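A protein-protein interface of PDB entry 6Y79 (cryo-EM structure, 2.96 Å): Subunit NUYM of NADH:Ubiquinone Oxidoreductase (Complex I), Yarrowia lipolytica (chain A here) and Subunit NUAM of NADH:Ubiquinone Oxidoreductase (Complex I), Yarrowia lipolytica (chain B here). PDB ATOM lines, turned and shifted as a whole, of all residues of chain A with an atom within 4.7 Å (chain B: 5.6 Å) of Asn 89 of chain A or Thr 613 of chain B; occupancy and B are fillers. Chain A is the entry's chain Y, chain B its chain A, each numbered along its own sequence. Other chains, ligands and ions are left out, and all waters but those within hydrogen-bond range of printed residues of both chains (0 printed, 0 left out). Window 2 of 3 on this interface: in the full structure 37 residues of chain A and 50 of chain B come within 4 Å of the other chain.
The backbone carbonyl oxygen of Gly 274 of chain B sits at hydrogen-bond distance from the side-chain hydroxyl of Thr 613 of chain B (2.8 Å).
The backbone carbonyl oxygen (O) of Thr 593 of chain B sits at hydrogen-bond distance from the backbone NH (N) of Ala 612 of chain B.
Among the printed residues, merely in contact across the chains: Ile 84 of chain A with Ala 611 of chain B (3.8 Å), Ile 84 of chain A with Ala 612 of chain B (3.6 Å), Ile 84 of chain A with Thr 613 of chain B (3.4 Å), Asn 89 of chain A with Gly 274 of chain B (3.8 Å), Asn 89 of chain A with Ala 612 of chain B (3.99 Å), Asn 89 of chain A with Thr 613 of chain B (3.9 Å), Arg 90 of chain A with Gly 274 of chain B (3.6 Å) and Arg 90 of chain A with Val 275 of chain B (3.6 Å).
Printed residues of chain B within 4 Å of Asn 89 of chain A: Gly 274 (3.8 Å), Ala 612 (3.99 Å) and Thr 613 (3.9 Å).
Gly 102 of chain A touches none of the printed residues of chain B.
Of the printed residues of chain A, Val 275 of chain B touches Arg 90.
Thr 593 of chain B touches none of the printed residues of chain A.
Of the printed residues of chain A, Ala 611 of chain B touches Ile 84.
Printed residues of chain A within 4 Å of Thr 613 of chain B: Ile 84 and Asn 89.
The nearest residue of chain A that does not touch Thr 613 of chain B is Asp 86 of chain A (4.4 Å).
Of the 13 printed residues of chain B, 5 touch a printed residue of chain A.
Printed residues of chain B that touch a printed residue of chain A: Gly 274, Val 275, Ala 611, Ala 612 and Thr 613.
Hydrophobic or aromatic side chains of chain B within 4 Å of the printed part of chain A: Val 275.
Hydrophobic or aromatic side chains of chain A within 4 Å of the printed part of chain B: Ile 84.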
ATOM      1  N   ILE A  84      -3.626  29.778   0.592  1.00  0.00           N
ATOM      2  CA  ILE A  84      -2.977  29.596  -0.695  1.00  0.00           C
ATOM      3  C   ILE A  84      -1.946  30.695  -0.934  1.00  0.00           C
ATOM      4  O   ILE A  84      -2.021  31.799  -0.388  1.00  0.00           O
ATOM      5  CB  ILE A  84      -4.011  29.533  -1.834  1.00  0.00           C
ATOM      6  CG1 ILE A  84      -4.706  30.874  -2.030  1.00  0.00           C
ATOM      7  CG2 ILE A  84      -5.045  28.468  -1.550  1.00  0.00           C
ATOM      8  CD1 ILE A  84      -5.627  30.882  -3.203  1.00  0.00           C
ATOM      9  N   VAL A  85      -0.946  30.353  -1.735  1.00  0.00           N
ATOM     10  CA  VAL A  85      -0.006  31.299  -2.317  1.00  0.00           C
ATOM     11  C   VAL A  85      -0.583  31.749  -3.646  1.00  0.00           C
ATOM     12  O   VAL A  85      -1.064  30.937  -4.423  1.00  0.00           O
ATOM     13  CB  VAL A  85       1.377  30.650  -2.498  1.00  0.00           C
ATOM     14  CG1 VAL A  85       2.390  31.662  -2.980  1.00  0.00           C
ATOM     15  CG2 VAL A  85       1.821  30.007  -1.210  1.00  0.00           C
ATOM     16  N   ASP A  86      -0.535  33.049  -3.919  1.00  0.00           N
ATOM     17  CA  ASP A  86      -1.263  33.591  -5.065  1.00  0.00           C
ATOM     18  C   ASP A  86      -0.540  33.347  -6.388  1.00  0.00           C
ATOM     19  O   ASP A  86      -1.188  33.235  -7.440  1.00  0.00           O
ATOM     20  CB  ASP A  86      -1.549  35.077  -4.845  1.00  0.00           C
ATOM     21  CG  ASP A  86      -2.655  35.298  -3.829  1.00  0.00           C
ATOM     22  OD1 ASP A  86      -3.428  34.345  -3.643  1.00  0.00           O
ATOM     23  OD2 ASP A  86      -2.776  36.397  -3.248  1.00  0.00           O
ATOM     24  N   VAL A  87       0.794  33.252  -6.359  1.00  0.00           N
ATOM     25  CA  VAL A  87       1.520  32.877  -7.570  1.00  0.00           C
ATOM     26  C   VAL A  87       1.604  31.362  -7.719  1.00  0.00           C
ATOM     27  O   VAL A  87       1.478  30.841  -8.833  1.00  0.00           O
ATOM     28  CB  VAL A  87       2.921  33.530  -7.621  1.00  0.00           C
ATOM     29  CG1 VAL A  87       3.823  33.126  -6.447  1.00  0.00           C
ATOM     30  CG2 VAL A  87       3.636  33.229  -8.949  1.00  0.00           C
ATOM     31  N   ALA A  88       1.727  30.634  -6.618  1.00  0.00           N
ATOM     32  CA  ALA A  88       2.023  29.214  -6.671  1.00  0.00           C
ATOM     33  C   ALA A  88       0.792  28.331  -6.591  1.00  0.00           C
ATOM     34  O   ALA A  88       0.954  27.110  -6.582  1.00  0.00           O
ATOM     35  CB  ALA A  88       2.976  28.823  -5.538  1.00  0.00           C
ATOM     36  N   ASN A  89      -0.419  28.898  -6.504  1.00  0.00           N
ATOM     37  CA  ASN A  89      -1.603  28.078  -6.248  1.00  0.00           C
ATOM     38  C   ASN A  89      -1.893  27.112  -7.378  1.00  0.00           C
ATOM     39  O   ASN A  89      -1.649  25.923  -7.215  1.00  0.00           O
ATOM     40  CB  ASN A  89      -2.876  28.891  -6.008  1.00  0.00           C
ATOM     41  CG  ASN A  89      -4.015  28.022  -5.517  1.00  0.00           C
ATOM     42  OD1 ASN A  89      -3.789  26.965  -4.925  1.00  0.00           O
ATOM     43  ND2 ASN A  89      -5.238  28.444  -5.776  1.00  0.00           N
ATOM     44  N   ARG A  90      -2.344  27.603  -8.530  1.00  0.00           N
ATOM     45  CA  ARG A  90      -2.706  26.764  -9.667  1.00  0.00           C
ATOM     46  C   ARG A  90      -2.639  27.573 -10.953  1.00  0.00           C
ATOM     47  O   ARG A  90      -2.948  28.767 -10.970  1.00  0.00           O
ATOM     48  CB  ARG A  90      -4.116  26.161  -9.556  1.00  0.00           C
ATOM     49  CG  ARG A  90      -4.249  24.936  -8.685  1.00  0.00           C
ATOM     50  CD  ARG A  90      -5.655  24.513  -8.564  1.00  0.00           C
ATOM     51  NE  ARG A  90      -5.883  23.674  -7.399  1.00  0.00           N
ATOM     52  CZ  ARG A  90      -5.738  22.362  -7.400  1.00  0.00           C
ATOM     53  NH1 ARG A  90      -5.402  21.748  -8.522  1.00  0.00           N
ATOM     54  NH2 ARG A  90      -5.951  21.665  -6.296  1.00  0.00           N
ATOM     55  N   TRP A  91      -2.244  26.903 -12.035  1.00  0.00           N
ATOM     56  CA  TRP A  91      -2.314  27.483 -13.368  1.00  0.00           C
ATOM     57  C   TRP A  91      -2.576  26.383 -14.383  1.00  0.00           C
ATOM     58  O   TRP A  91      -2.234  25.223 -14.158  1.00  0.00           O
ATOM     59  CB  TRP A  91      -1.039  28.244 -13.743  1.00  0.00           C
ATOM     60  CG  TRP A  91       0.211  27.428 -13.778  1.00  0.00           C
ATOM     61  CD1 TRP A  91       0.780  26.852 -14.866  1.00  0.00           C
ATOM     62  CD2 TRP A  91       1.063  27.129 -12.674  1.00  0.00           C
ATOM     63  NE1 TRP A  91       1.928  26.201 -14.508  1.00  0.00           N
ATOM     64  CE2 TRP A  91       2.121  26.354 -13.163  1.00  0.00           C
ATOM     65  CE3 TRP A  91       1.022  27.428 -11.314  1.00  0.00           C
ATOM     66  CZ2 TRP A  91       3.131  25.881 -12.346  1.00  0.00           C
ATOM     67  CZ3 TRP A  91       2.026  26.959 -10.507  1.00  0.00           C
ATOM     68  CH2 TRP A  91       3.069  26.199 -11.024  1.00  0.00           C
ATOM     69  N   SER A 100      -1.894  22.659 -13.085  1.00  0.00           N
ATOM     70  CA  SER A 100      -0.548  22.501 -12.555  1.00  0.00           C
ATOM     71  C   SER A 100      -0.382  23.365 -11.318  1.00  0.00           C
ATOM     72  O   SER A 100      -1.022  24.403 -11.189  1.00  0.00           O
ATOM     73  CB  SER A 100       0.496  22.908 -13.586  1.00  0.00           C
ATOM     74  OG  SER A 100       0.382  22.130 -14.753  1.00  0.00           O
ATOM     75  N   SER A 101       0.484  22.945 -10.408  1.00  0.00           N
ATOM     76  CA  SER A 101       0.670  23.683  -9.171  1.00  0.00           C
ATOM     77  C   SER A 101       2.109  23.581  -8.689  1.00  0.00           C
ATOM     78  O   SER A 101       2.792  22.579  -8.894  1.00  0.00           O
ATOM     79  CB  SER A 101      -0.269  23.186  -8.071  1.00  0.00           C
ATOM     80  OG  SER A 101       0.158  21.972  -7.505  1.00  0.00           O
ATOM     81  N   GLY A 102       2.554  24.632  -8.012  1.00  0.00           N
ATOM     82  CA  GLY A 102       3.841  24.636  -7.352  1.00  0.00           C
ATOM     83  C   GLY A 102       3.686  24.655  -5.848  1.00  0.00           C
ATOM     84  O   GLY A 102       4.634  24.371  -5.113  1.00  0.00           O
ATOM     85  N   ASP A 103       2.494  25.012  -5.381  1.00  0.00           N
ATOM     86  CA  ASP A 103       2.160  24.851  -3.974  1.00  0.00           C
ATOM     87  C   ASP A 103       1.939  23.377  -3.682  1.00  0.00           C
ATOM     88  O   ASP A 103       1.190  22.701  -4.390  1.00  0.00           O
ATOM     89  CB  ASP A 103       0.909  25.654  -3.621  1.00  0.00           C
ATOM     90  CG  ASP A 103       0.686  25.771  -2.126  1.00  0.00           C
ATOM     91  OD1 ASP A 103       1.552  25.331  -1.345  1.00  0.00           O
ATOM     92  OD2 ASP A 103      -0.367  26.309  -1.727  1.00  0.00           O
ATOM     93  N   SER B 272     -14.544  25.663  -5.702  1.00  0.00           N
ATOM     94  CA  SER B 272     -13.583  25.972  -6.744  1.00  0.00           C
ATOM     95  C   SER B 272     -13.014  24.693  -7.333  1.00  0.00           C
ATOM     96  O   SER B 272     -12.635  23.774  -6.600  1.00  0.00           O
ATOM     97  CB  SER B 272     -12.442  26.838  -6.201  1.00  0.00           C
ATOM     98  OG  SER B 272     -12.912  28.111  -5.798  1.00  0.00           O
ATOM     99  N   GLY B 274     -10.343  25.276  -8.999  1.00  0.00           N
ATOM    100  CA  GLY B 274      -9.043  25.708  -8.536  1.00  0.00           C
ATOM    101  C   GLY B 274      -8.472  26.923  -9.237  1.00  0.00           C
ATOM    102  O   GLY B 274      -7.664  27.654  -8.657  1.00  0.00           O
ATOM    103  N   VAL B 275      -8.862  27.148 -10.486  1.00  0.00           N
ATOM    104  CA  VAL B 275      -8.555  28.409 -11.151  1.00  0.00           C
ATOM    105  C   VAL B 275      -9.892  29.076 -11.445  1.00  0.00           C
ATOM    106  O   VAL B 275     -10.024  30.303 -11.361  1.00  0.00           O
ATOM    107  CB  VAL B 275      -7.688  28.194 -12.408  1.00  0.00           C
ATOM    108  CG1 VAL B 275      -7.566  29.453 -13.240  1.00  0.00           C
ATOM    109  CG2 VAL B 275      -6.300  27.793 -11.998  1.00  0.00           C
ATOM    110  N   GLU B 276     -10.910  28.261 -11.695  1.00  0.00           N
ATOM    111  CA  GLU B 276     -12.267  28.752 -11.875  1.00  0.00           C
ATOM    112  C   GLU B 276     -13.066  28.641 -10.582  1.00  0.00           C
ATOM    113  O   GLU B 276     -12.719  27.893  -9.665  1.00  0.00           O
ATOM    114  CB  GLU B 276     -12.987  27.969 -12.968  1.00  0.00           C
ATOM    115  CG  GLU B 276     -12.493  28.163 -14.385  1.00  0.00           C
ATOM    116  CD  GLU B 276     -13.289  27.318 -15.364  1.00  0.00           C
ATOM    117  OE1 GLU B 276     -14.063  26.467 -14.891  1.00  0.00           O
ATOM    118  OE2 GLU B 276     -13.172  27.509 -16.594  1.00  0.00           O
ATOM    119  N   VAL B 277     -14.169  29.384 -10.535  1.00  0.00           N
ATOM    120  CA  VAL B 277     -15.077  29.414  -9.395  1.00  0.00           C
ATOM    121  C   VAL B 277     -16.439  28.936  -9.868  1.00  0.00           C
ATOM    122  O   VAL B 277     -16.960  29.430 -10.872  1.00  0.00           O
ATOM    123  CB  VAL B 277     -15.160  30.822  -8.787  1.00  0.00           C
ATOM    124  CG1 VAL B 277     -16.204  30.889  -7.683  1.00  0.00           C
ATOM    125  CG2 VAL B 277     -13.805  31.222  -8.271  1.00  0.00           C
ATOM    126  N   THR B 593     -13.008  36.982  -4.433  1.00  0.00           N
ATOM    127  CA  THR B 593     -12.673  35.570  -4.325  1.00  0.00           C
ATOM    128  C   THR B 593     -11.168  35.363  -4.212  1.00  0.00           C
ATOM    129  O   THR B 593     -10.706  34.542  -3.414  1.00  0.00           O
ATOM    130  CB  THR B 593     -13.225  34.821  -5.536  1.00  0.00           C
ATOM    131  OG1 THR B 593     -14.644  34.995  -5.599  1.00  0.00           O
ATOM    132  CG2 THR B 593     -12.930  33.359  -5.430  1.00  0.00           C
ATOM    133  N   GLU B 594     -10.390  36.130  -4.967  1.00  0.00           N
ATOM    134  CA  GLU B 594      -8.963  35.894  -5.129  1.00  0.00           C
ATOM    135  C   GLU B 594      -8.116  36.488  -4.012  1.00  0.00           C
ATOM    136  O   GLU B 594      -6.890  36.351  -4.054  1.00  0.00           O
ATOM    137  CB  GLU B 594      -8.500  36.451  -6.479  1.00  0.00           C
ATOM    138  CG  GLU B 594      -9.056  35.720  -7.700  1.00  0.00           C
ATOM    139  CD  GLU B 594     -10.437  36.196  -8.103  1.00  0.00           C
ATOM    140  OE1 GLU B 594     -10.945  37.131  -7.458  1.00  0.00           O
ATOM    141  OE2 GLU B 594     -11.017  35.634  -9.057  1.00  0.00           O
ATOM    142  N   LYS B 595      -8.722  37.140  -3.024  1.00  0.00           N
ATOM    143  CA  LYS B 595      -7.964  37.768  -1.957  1.00  0.00           C
ATOM    144  C   LYS B 595      -8.639  37.514  -0.617  1.00  0.00           C
ATOM    145  O   LYS B 595      -9.858  37.338  -0.535  1.00  0.00           O
ATOM    146  CB  LYS B 595      -7.802  39.278  -2.208  1.00  0.00           C
ATOM    147  CG  LYS B 595      -9.095  40.075  -2.191  1.00  0.00           C
ATOM    148  CD  LYS B 595      -8.844  41.525  -2.550  1.00  0.00           C
ATOM    149  CE  LYS B 595     -10.111  42.355  -2.448  1.00  0.00           C
ATOM    150  NZ  LYS B 595      -9.814  43.750  -2.024  1.00  0.00           N
ATOM    151  N   ALA B 611      -9.211  33.576   0.585  1.00  0.00           N
ATOM    152  CA  ALA B 611      -8.973  33.485  -0.846  1.00  0.00           C
ATOM    153  C   ALA B 611      -9.191  32.055  -1.319  1.00  0.00           C
ATOM    154  O   ALA B 611      -8.575  31.122  -0.796  1.00  0.00           O
ATOM    155  CB  ALA B 611      -7.557  33.940  -1.182  1.00  0.00           C
ATOM    156  N   ALA B 612     -10.067  31.884  -2.306  1.00  0.00           N
ATOM    157  CA  ALA B 612     -10.319  30.560  -2.863  1.00  0.00           C
ATOM    158  C   ALA B 612      -9.330  30.213  -3.969  1.00  0.00           C
ATOM    159  O   ALA B 612      -8.710  29.147  -3.941  1.00  0.00           O
ATOM    160  CB  ALA B 612     -11.748  30.473  -3.391  1.00  0.00           C
ATOM    161  N   THR B 613      -9.172  31.102  -4.939  1.00  0.00           N
ATOM    162  CA  THR B 613      -8.255  30.923  -6.055  1.00  0.00           C
ATOM    163  C   THR B 613      -7.300  32.110  -6.123  1.00  0.00           C
ATOM    164  O   THR B 613      -7.328  33.007  -5.280  1.00  0.00           O
ATOM    165  CB  THR B 613      -9.027  30.754  -7.370  1.00  0.00           C
ATOM    166  OG1 THR B 613      -8.114  30.449  -8.430  1.00  0.00           O
ATOM    167  CG2 THR B 613      -9.798  32.019  -7.712  1.00  0.00           C
ATOM    168  N   GLY B 614      -6.435  32.103  -7.131  1.00  0.00           N
ATOM    169  CA  GLY B 614      -5.513  33.191  -7.340  1.00  0.00           C
ATOM    170  C   GLY B 614      -5.990  34.123  -8.433  1.00  0.00           C
ATOM    171  O   GLY B 614      -6.850  33.770  -9.247  1.00  0.00           O
ATOM    172  N   PRO B 615      -5.465  35.345  -8.457  1.00  0.00           N
ATOM    173  CA  PRO B 615      -5.788  36.285  -9.538  1.00  0.00           C
ATOM    174  C   PRO B 615      -5.245  35.804 -10.861  1.00  0.00           C
ATOM    175  O   PRO B 615      -4.047  35.483 -10.975  1.00  0.00           O
ATOM    176  CB  PRO B 615      -5.103  37.584  -9.086  1.00  0.00           C
ATOM    177  CG  PRO B 615      -4.992  37.455  -7.619  1.00  0.00           C
ATOM    178  CD  PRO B 615      -4.745  36.006  -7.358  1.00  0.00           C
